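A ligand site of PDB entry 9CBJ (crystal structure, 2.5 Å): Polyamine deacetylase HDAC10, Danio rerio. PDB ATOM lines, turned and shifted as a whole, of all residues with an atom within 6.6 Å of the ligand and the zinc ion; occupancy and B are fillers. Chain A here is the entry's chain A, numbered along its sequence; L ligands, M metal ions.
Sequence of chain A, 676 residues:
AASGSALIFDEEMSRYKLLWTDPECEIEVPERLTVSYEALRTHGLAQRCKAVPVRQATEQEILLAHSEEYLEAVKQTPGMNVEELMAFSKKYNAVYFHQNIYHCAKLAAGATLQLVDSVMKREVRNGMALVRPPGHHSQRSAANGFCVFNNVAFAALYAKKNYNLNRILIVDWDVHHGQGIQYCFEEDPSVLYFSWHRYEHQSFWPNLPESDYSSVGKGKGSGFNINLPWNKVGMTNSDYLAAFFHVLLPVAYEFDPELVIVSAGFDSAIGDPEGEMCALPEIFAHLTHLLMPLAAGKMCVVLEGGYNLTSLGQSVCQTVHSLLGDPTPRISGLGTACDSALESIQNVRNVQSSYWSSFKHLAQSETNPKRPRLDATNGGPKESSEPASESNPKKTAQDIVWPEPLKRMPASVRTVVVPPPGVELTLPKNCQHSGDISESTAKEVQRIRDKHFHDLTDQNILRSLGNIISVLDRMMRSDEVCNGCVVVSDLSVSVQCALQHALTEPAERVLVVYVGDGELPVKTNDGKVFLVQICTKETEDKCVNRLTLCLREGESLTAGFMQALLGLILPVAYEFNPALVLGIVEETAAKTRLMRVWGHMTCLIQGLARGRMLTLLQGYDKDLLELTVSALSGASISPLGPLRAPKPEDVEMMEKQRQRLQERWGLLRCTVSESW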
ATOM      1  N   GLU A  24       1.436  22.967   7.028  1.00  0.00           N
ATOM      2  CA  GLU A  24       0.488  21.878   6.832  1.00  0.00           C
ATOM      3  C   GLU A  24       0.947  20.913   5.760  1.00  0.00           C
ATOM      4  O   GLU A  24       0.710  19.698   5.867  1.00  0.00           O
ATOM      5  CB  GLU A  24      -0.874  22.464   6.480  1.00  0.00           C
ATOM      6  CG  GLU A  24      -2.060  21.591   6.801  1.00  0.00           C
ATOM      7  CD  GLU A  24      -3.372  22.314   6.582  1.00  0.00           C
ATOM      8  OE1 GLU A  24      -3.446  23.126   5.636  1.00  0.00           O
ATOM      9  OE2 GLU A  24      -4.313  22.083   7.375  1.00  0.00           O
ATOM     10  N   CYS A  25       1.627  21.416   4.727  1.00  0.00           N
ATOM     11  CA  CYS A  25       2.011  20.611   3.576  1.00  0.00           C
ATOM     12  C   CYS A  25       3.511  20.339   3.491  1.00  0.00           C
ATOM     13  O   CYS A  25       3.943  19.669   2.559  1.00  0.00           O
ATOM     14  CB  CYS A  25       1.548  21.279   2.281  1.00  0.00           C
ATOM     15  SG  CYS A  25      -0.228  21.529   2.151  1.00  0.00           S
ATOM     16  N   ILE A  27       5.383  18.323   4.720  1.00  0.00           N
ATOM     17  CA  ILE A  27       5.792  16.925   4.773  1.00  0.00           C
ATOM     18  C   ILE A  27       5.739  16.261   3.393  1.00  0.00           C
ATOM     19  O   ILE A  27       6.493  15.324   3.127  1.00  0.00           O
ATOM     20  CB  ILE A  27       4.938  16.157   5.780  1.00  0.00           C
ATOM     21  CG1 ILE A  27       3.451  16.414   5.518  1.00  0.00           C
ATOM     22  CG2 ILE A  27       5.323  16.531   7.205  1.00  0.00           C
ATOM     23  CD1 ILE A  27       2.522  15.560   6.341  1.00  0.00           C
ATOM     24  N   ASN A  93      -8.524  22.583   1.055  1.00  0.00           N
ATOM     25  CA  ASN A  93      -8.002  22.288   2.386  1.00  0.00           C
ATOM     26  C   ASN A  93      -6.771  21.390   2.290  1.00  0.00           C
ATOM     27  O   ASN A  93      -6.838  20.315   1.673  1.00  0.00           O
ATOM     28  CB  ASN A  93      -9.065  21.634   3.260  1.00  0.00           C
ATOM     29  CG  ASN A  93      -8.562  21.297   4.647  1.00  0.00           C
ATOM     30  OD1 ASN A  93      -8.774  20.196   5.151  1.00  0.00           O
ATOM     31  ND2 ASN A  93      -7.878  22.246   5.268  1.00  0.00           N
ATOM     32  N   ALA A  94      -5.670  21.830   2.896  1.00  0.00           N
ATOM     33  CA  ALA A  94      -4.435  21.045   3.000  1.00  0.00           C
ATOM     34  C   ALA A  94      -3.917  20.645   1.623  1.00  0.00           C
ATOM     35  O   ALA A  94      -3.626  19.475   1.359  1.00  0.00           O
ATOM     36  CB  ALA A  94      -4.632  19.821   3.900  1.00  0.00           C
ATOM     37  N   PRO A 134      -0.754  11.761  -4.166  1.00  0.00           N
ATOM     38  CA  PRO A 134      -1.717  10.732  -3.742  1.00  0.00           C
ATOM     39  C   PRO A 134      -3.121  11.089  -4.189  1.00  0.00           C
ATOM     40  O   PRO A 134      -3.341  12.150  -4.764  1.00  0.00           O
ATOM     41  CB  PRO A 134      -1.580  10.721  -2.217  1.00  0.00           C
ATOM     42  CG  PRO A 134      -1.092  12.088  -1.881  1.00  0.00           C
ATOM     43  CD  PRO A 134      -0.186  12.486  -3.012  1.00  0.00           C
ATOM     44  N   HIS A 136      -6.490   9.560  -2.450  1.00  0.00           N
ATOM     45  CA  HIS A 136      -7.693   9.074  -1.779  1.00  0.00           C
ATOM     46  C   HIS A 136      -8.494  10.159  -1.059  1.00  0.00           C
ATOM     47  O   HIS A 136      -9.608   9.880  -0.615  1.00  0.00           O
ATOM     48  CB  HIS A 136      -7.337   7.938  -0.807  1.00  0.00           C
ATOM     49  CG  HIS A 136      -6.543   8.366   0.387  1.00  0.00           C
ATOM     50  ND1 HIS A 136      -6.642   7.725   1.608  1.00  0.00           N
ATOM     51  CD2 HIS A 136      -5.627   9.351   0.556  1.00  0.00           C
ATOM     52  CE1 HIS A 136      -5.815   8.300   2.473  1.00  0.00           C
ATOM     53  NE2 HIS A 136      -5.193   9.289   1.861  1.00  0.00           N
ATOM     54  N   HIS A 137      -7.975  11.384  -0.952  1.00  0.00           N
ATOM     55  CA  HIS A 137      -8.743  12.471  -0.352  1.00  0.00           C
ATOM     56  C   HIS A 137      -9.427  13.358  -1.384  1.00  0.00           C
ATOM     57  O   HIS A 137     -10.320  14.135  -1.017  1.00  0.00           O
ATOM     58  CB  HIS A 137      -7.846  13.346   0.530  1.00  0.00           C
ATOM     59  CG  HIS A 137      -7.331  12.649   1.746  1.00  0.00           C
ATOM     60  ND1 HIS A 137      -8.165  12.154   2.739  1.00  0.00           N
ATOM     61  CD2 HIS A 137      -6.070  12.377   2.148  1.00  0.00           C
ATOM     62  CE1 HIS A 137      -7.434  11.595   3.684  1.00  0.00           C
ATOM     63  NE2 HIS A 137      -6.155  11.719   3.358  1.00  0.00           N
ATOM     64  N   ASN A 144      -7.968  17.945  -2.191  1.00  0.00           N
ATOM     65  CA  ASN A 144      -8.052  17.852  -0.734  1.00  0.00           C
ATOM     66  C   ASN A 144      -6.929  16.966  -0.227  1.00  0.00           C
ATOM     67  O   ASN A 144      -6.641  15.924  -0.811  1.00  0.00           O
ATOM     68  CB  ASN A 144      -9.412  17.295  -0.297  1.00  0.00           C
ATOM     69  CG  ASN A 144      -9.641  17.437   1.183  1.00  0.00           C
ATOM     70  OD1 ASN A 144      -9.345  16.534   1.962  1.00  0.00           O
ATOM     71  ND2 ASN A 144     -10.172  18.584   1.598  1.00  0.00           N
ATOM     72  N   GLY A 145      -6.294  17.400   0.863  1.00  0.00           N
ATOM     73  CA  GLY A 145      -5.288  16.604   1.552  1.00  0.00           C
ATOM     74  C   GLY A 145      -4.194  16.030   0.662  1.00  0.00           C
ATOM     75  O   GLY A 145      -4.055  14.812   0.565  1.00  0.00           O
ATOM     76  N   PHE A 146      -3.434  16.915   0.018  1.00  0.00           N
ATOM     77  CA  PHE A 146      -2.317  16.577  -0.870  1.00  0.00           C
ATOM     78  C   PHE A 146      -2.752  15.865  -2.145  1.00  0.00           C
ATOM     79  O   PHE A 146      -1.897  15.437  -2.925  1.00  0.00           O
ATOM     80  CB  PHE A 146      -1.250  15.708  -0.186  1.00  0.00           C
ATOM     81  CG  PHE A 146      -0.762  16.223   1.149  1.00  0.00           C
ATOM     82  CD1 PHE A 146      -0.936  17.549   1.520  1.00  0.00           C
ATOM     83  CD2 PHE A 146      -0.121  15.371   2.036  1.00  0.00           C
ATOM     84  CE1 PHE A 146      -0.504  18.004   2.753  1.00  0.00           C
ATOM     85  CE2 PHE A 146       0.326  15.818   3.263  1.00  0.00           C
ATOM     86  CZ  PHE A 146       0.137  17.136   3.628  1.00  0.00           C
ATOM     87  N   CYS A 147      -4.059  15.730  -2.387  1.00  0.00           N
ATOM     88  CA  CYS A 147      -4.569  14.922  -3.482  1.00  0.00           C
ATOM     89  C   CYS A 147      -5.268  15.801  -4.504  1.00  0.00           C
ATOM     90  O   CYS A 147      -6.086  16.648  -4.150  1.00  0.00           O
ATOM     91  CB  CYS A 147      -5.538  13.858  -2.962  1.00  0.00           C
ATOM     92  SG  CYS A 147      -4.794  12.699  -1.785  1.00  0.00           S
ATOM     93  N   ASP A 174      -3.868   3.553   4.571  1.00  0.00           N
ATOM     94  CA  ASP A 174      -3.336   4.846   4.970  1.00  0.00           C
ATOM     95  C   ASP A 174      -3.917   5.245   6.316  1.00  0.00           C
ATOM     96  O   ASP A 174      -5.014   4.824   6.698  1.00  0.00           O
ATOM     97  CB  ASP A 174      -3.650   5.893   3.900  1.00  0.00           C
ATOM     98  CG  ASP A 174      -2.912   7.207   4.117  1.00  0.00           C
ATOM     99  OD1 ASP A 174      -3.210   7.907   5.107  1.00  0.00           O
ATOM    100  OD2 ASP A 174      -2.049   7.541   3.288  1.00  0.00           O
ATOM    101  N   VAL A 175      -3.166   6.060   7.063  1.00  0.00           N
ATOM    102  CA  VAL A 175      -3.606   6.437   8.402  1.00  0.00           C
ATOM    103  C   VAL A 175      -4.719   7.468   8.368  1.00  0.00           C
ATOM    104  O   VAL A 175      -5.401   7.681   9.381  1.00  0.00           O
ATOM    105  CB  VAL A 175      -2.426   6.948   9.245  1.00  0.00           C
ATOM    106  CG1 VAL A 175      -2.156   8.420   8.962  1.00  0.00           C
ATOM    107  CG2 VAL A 175      -2.680   6.711  10.731  1.00  0.00           C
ATOM    108  N   HIS A 176      -4.942   8.117   7.227  1.00  0.00           N
ATOM    109  CA  HIS A 176      -6.041   9.061   7.075  1.00  0.00           C
ATOM    110  C   HIS A 176      -7.212   8.394   6.373  1.00  0.00           C
ATOM    111  O   HIS A 176      -7.051   7.398   5.646  1.00  0.00           O
ATOM    112  CB  HIS A 176      -5.592  10.303   6.295  1.00  0.00           C
ATOM    113  CG  HIS A 176      -4.500  11.073   6.963  1.00  0.00           C
ATOM    114  ND1 HIS A 176      -3.160  10.782   6.790  1.00  0.00           N
ATOM    115  CD2 HIS A 176      -4.548  12.134   7.800  1.00  0.00           C
ATOM    116  CE1 HIS A 176      -2.435  11.624   7.502  1.00  0.00           C
ATOM    117  NE2 HIS A 176      -3.250  12.455   8.128  1.00  0.00           N
ATOM    118  N   HIS A 177      -8.400   8.939   6.588  1.00  0.00           N
ATOM    119  CA  HIS A 177      -9.613   8.384   6.002  1.00  0.00           C
ATOM    120  C   HIS A 177      -9.761   8.883   4.576  1.00  0.00           C
ATOM    121  O   HIS A 177      -9.952  10.084   4.348  1.00  0.00           O
ATOM    122  CB  HIS A 177     -10.833   8.749   6.824  1.00  0.00           C
ATOM    123  CG  HIS A 177     -12.121   8.276   6.232  1.00  0.00           C
ATOM    124  ND1 HIS A 177     -13.184   9.120   5.963  1.00  0.00           N
ATOM    125  CD2 HIS A 177     -12.514   7.046   5.811  1.00  0.00           C
ATOM    126  CE1 HIS A 177     -14.165   8.431   5.436  1.00  0.00           C
ATOM    127  NE2 HIS A 177     -13.793   7.166   5.329  1.00  0.00           N
ATOM    128  N   PHE A 204      -9.337  14.318  14.763  1.00  0.00           N
ATOM    129  CA  PHE A 204      -8.219  14.252  13.830  1.00  0.00           C
ATOM    130  C   PHE A 204      -8.696  14.515  12.407  1.00  0.00           C
ATOM    131  O   PHE A 204      -9.823  14.180  12.028  1.00  0.00           O
ATOM    132  CB  PHE A 204      -7.519  12.894  13.907  1.00  0.00           C
ATOM    133  CG  PHE A 204      -6.229  12.851  13.138  1.00  0.00           C
ATOM    134  CD1 PHE A 204      -5.111  13.540  13.596  1.00  0.00           C
ATOM    135  CD2 PHE A 204      -6.125  12.108  11.977  1.00  0.00           C
ATOM    136  CE1 PHE A 204      -3.923  13.501  12.892  1.00  0.00           C
ATOM    137  CE2 PHE A 204      -4.937  12.068  11.273  1.00  0.00           C
ATOM    138  CZ  PHE A 204      -3.833  12.758  11.731  1.00  0.00           C
ATOM    139  N   TRP A 205      -7.816  15.113  11.610  1.00  0.00           N
ATOM    140  CA  TRP A 205      -8.149  15.483  10.243  1.00  0.00           C
ATOM    141  C   TRP A 205      -8.520  14.244   9.436  1.00  0.00           C
ATOM    142  O   TRP A 205      -7.864  13.197   9.566  1.00  0.00           O
ATOM    143  CB  TRP A 205      -6.964  16.206   9.606  1.00  0.00           C
ATOM    144  CG  TRP A 205      -7.287  16.868   8.316  1.00  0.00           C
ATOM    145  CD1 TRP A 205      -7.624  18.176   8.131  1.00  0.00           C
ATOM    146  CD2 TRP A 205      -7.313  16.257   7.032  1.00  0.00           C
ATOM    147  NE1 TRP A 205      -7.864  18.418   6.798  1.00  0.00           N
ATOM    148  CE2 TRP A 205      -7.684  17.249   6.103  1.00  0.00           C
ATOM    149  CE3 TRP A 205      -7.077  14.956   6.561  1.00  0.00           C
ATOM    150  CZ2 TRP A 205      -7.805  16.988   4.738  1.00  0.00           C
ATOM    151  CZ3 TRP A 205      -7.198  14.703   5.219  1.00  0.00           C
ATOM    152  CH2 TRP A 205      -7.563  15.715   4.313  1.00  0.00           C
ATOM    153  N   GLY A 265      -0.954   3.641   1.930  1.00  0.00           N
ATOM    154  CA  GLY A 265      -0.406   4.774   2.625  1.00  0.00           C
ATOM    155  C   GLY A 265       0.361   4.295   3.829  1.00  0.00           C
ATOM    156  O   GLY A 265      -0.193   3.635   4.718  1.00  0.00           O
ATOM    157  N   ASP A 267       1.938   6.191   6.067  1.00  0.00           N
ATOM    158  CA  ASP A 267       1.923   7.060   7.241  1.00  0.00           C
ATOM    159  C   ASP A 267       1.258   6.396   8.438  1.00  0.00           C
ATOM    160  O   ASP A 267       1.104   7.042   9.479  1.00  0.00           O
ATOM    161  CB  ASP A 267       1.232   8.384   6.909  1.00  0.00           C
ATOM    162  CG  ASP A 267      -0.102   8.190   6.213  1.00  0.00           C
ATOM    163  OD1 ASP A 267      -0.538   7.033   6.047  1.00  0.00           O
ATOM    164  OD2 ASP A 267      -0.715   9.205   5.840  1.00  0.00           O
ATOM    165  N   GLU A 274       2.649  12.065  11.104  1.00  0.00           N
ATOM    166  CA  GLU A 274       1.230  12.333  10.926  1.00  0.00           C
ATOM    167  C   GLU A 274       0.349  11.289  11.601  1.00  0.00           C
ATOM    168  O   GLU A 274      -0.679  11.636  12.193  1.00  0.00           O
ATOM    169  CB  GLU A 274       0.890  12.421   9.435  1.00  0.00           C
ATOM    170  CG  GLU A 274      -0.013  13.580   9.060  1.00  0.00           C
ATOM    171  CD  GLU A 274       0.657  14.923   9.241  1.00  0.00           C
ATOM    172  OE1 GLU A 274       1.900  14.970   9.385  1.00  0.00           O
ATOM    173  OE2 GLU A 274      -0.062  15.952   9.252  1.00  0.00           O
ATOM    174  N   GLU A 304      -0.015   6.087  -1.426  1.00  0.00           N
ATOM    175  CA  GLU A 304      -0.753   7.246  -0.956  1.00  0.00           C
ATOM    176  C   GLU A 304       0.156   8.087  -0.063  1.00  0.00           C
ATOM    177  O   GLU A 304       1.030   8.791  -0.568  1.00  0.00           O
ATOM    178  CB  GLU A 304      -2.014   6.825  -0.187  1.00  0.00           C
ATOM    179  CG  GLU A 304      -2.984   5.976  -1.002  1.00  0.00           C
ATOM    180  CD  GLU A 304      -3.925   6.808  -1.855  1.00  0.00           C
ATOM    181  OE1 GLU A 304      -3.917   8.046  -1.722  1.00  0.00           O
ATOM    182  OE2 GLU A 304      -4.679   6.207  -2.654  1.00  0.00           O
ATOM    183  N   GLY A 305      -0.014   7.990   1.251  1.00  0.00           N
ATOM    184  CA  GLY A 305       0.756   8.766   2.200  1.00  0.00           C
ATOM    185  C   GLY A 305       2.033   8.072   2.615  1.00  0.00           C
ATOM    186  O   GLY A 305       2.472   7.085   2.004  1.00  0.00           O
ATOM    187  N   GLY A 306       2.636   8.577   3.694  1.00  0.00           N
ATOM    188  CA  GLY A 306       3.905   8.077   4.183  1.00  0.00           C
ATOM    189  C   GLY A 306       4.983   9.140   4.095  1.00  0.00           C
ATOM    190  O   GLY A 306       5.412   9.497   2.995  1.00  0.00           O
ATOM    191  N   TYR A 307       5.456   9.633   5.244  1.00  0.00           N
ATOM    192  CA  TYR A 307       6.262  10.848   5.258  1.00  0.00           C
ATOM    193  C   TYR A 307       7.551  10.755   6.054  1.00  0.00           C
ATOM    194  O   TYR A 307       8.375  11.670   5.952  1.00  0.00           O
ATOM    195  CB  TYR A 307       5.416  12.023   5.777  1.00  0.00           C
ATOM    196  CG  TYR A 307       4.121  12.136   4.987  1.00  0.00           C
ATOM    197  CD1 TYR A 307       4.113  12.730   3.731  1.00  0.00           C
ATOM    198  CD2 TYR A 307       2.937  11.606   5.467  1.00  0.00           C
ATOM    199  CE1 TYR A 307       2.949  12.815   2.992  1.00  0.00           C
ATOM    200  CE2 TYR A 307       1.766  11.696   4.740  1.00  0.00           C
ATOM    201  CZ  TYR A 307       1.779  12.300   3.502  1.00  0.00           C
ATOM    202  OH  TYR A 307       0.622  12.390   2.758  1.00  0.00           O
HETATM  203  C1  LIG L   1      -2.745  12.830   3.141  1.00  0.00           C
HETATM  204  C2  LIG L   1      -2.082  13.285   4.435  1.00  0.00           C
HETATM  205  C3  LIG L   1      -2.433  14.572   5.127  1.00  0.00           C
HETATM  206  C4  LIG L   1      -1.617  15.141   6.102  1.00  0.00           C
HETATM  207  C5  LIG L   1      -1.956  16.347   6.751  1.00  0.00           C
HETATM  208  C6  LIG L   1      -3.131  17.069   6.481  1.00  0.00           C
HETATM  209  C7  LIG L   1      -3.491  18.368   7.207  1.00  0.00           C
HETATM  210  C8  LIG L   1      -4.135  18.207   8.616  1.00  0.00           C
HETATM  211  C9  LIG L   1      -3.575  19.080   9.790  1.00  0.00           C
HETATM  212  C10 LIG L   1      -3.962  16.477   5.488  1.00  0.00           C
HETATM  213  C11 LIG L   1      -3.637  15.264   4.831  1.00  0.00           C
HETATM  214  N1  LIG L   1      -3.597  20.529   9.494  1.00  0.00           N
HETATM  215  O1  LIG L   1      -1.208  12.533   4.936  1.00  0.00           O
HETATM  216  S1  LIG L   1      -2.489  11.021   2.830  1.00  0.00           S
HETATM  217 ZN    ZN M   1      -2.333   9.837   4.867  1.00  0.00          ZN
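OD2 of Asp 267 binds the zinc ion, 2.0 Å away.
The side-chain carboxylate (OD1) of Asp 174 binds the zinc ion, at 2.1 Å.
ND1 of His 176 is bound to the zinc ion (2.3 Å).
A sulfur (S1) of the ligand binds the zinc ion (2.4 Å).
Slightly farther from the zinc ion lies the side-chain carboxylate (OD2) of Asp 174 (2.8 Å).
The backbone NH (N) of Phe 146 is in hydrogen-bond range of the backbone carbonyl oxygen (O) of Ala 94, at 2.9 Å.
OD1 of Asn 93 is in hydrogen-bond range of NE1 of Trp 205 (2.6 Å).
The backbone NH (N) of His 136 lies within hydrogen-bond range of the side-chain carboxylate (OE1) of Glu 304 (3.1 Å).
The side-chain carboxylate (OD1) of Asp 267 sits at hydrogen-bond distance from the backbone NH (N) of Val 175, 3.0 Å away.
NE2 of His 136 lies within hydrogen-bond range of NE2 of His 137, 3.0 Å away.
The backbone carbonyl oxygen (O) of Gly 145 lies within hydrogen-bond range of the side-chain sulfur (SG) of Cys 147 (3.2 Å).
The backbone NH (N) of Gly 145 lies within hydrogen-bond range of the backbone carbonyl oxygen (O) of Asn 93.
N of Gly 305 is in hydrogen-bond range of OD2 of Asp 174 (2.9 Å).
Ala 94 touches the ligand (CB to C10, 3.8 Å).
Gly 145 touches the ligand (O to C1, 3.5 Å).
Phe 146 touches the ligand (CE2 to C4, 3.5 Å).
CG of Trp 205 touches C8 of the ligand (3.4 Å).
OE2 of Glu 274 touches C5 of the ligand, at 3.2 Å.
Hydrophobic or aromatic side chains within 4 Å of the ligand: Ala 94, His 137, Phe 146, His 176, Trp 205 and Tyr 307.
Within 4 Å of the ligand: Glu 24, Ala 94, His 136, His 137, Gly 145, Phe 146, Asp 174, His 176, Trp 205, Asp 267, Glu 274 and Tyr 307.
Along chain A the residues within 4 Å of the ligand span positions 24 to 307.
OE2 of Glu 24 lies within salt-bridge range of N1 of the ligand.
A ring nitrogen (NE2) of His 137 sits close to a sulfur (S1) of the ligand.
The side-chain hydroxyl of Tyr 307 sits at hydrogen-bond distance from an oxygen (O1) of the ligand (2.8 Å).
A ring nitrogen (NE2) of His 136 sits close to a sulfur (S1) of the ligand (3.4 Å).
Three residues have an atom within 4 Å of the zinc ion: Asp 174, His 176 and Asp 267.
The nearest printed residue that does not touch the zinc ion is His 136 (4.2 Å).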
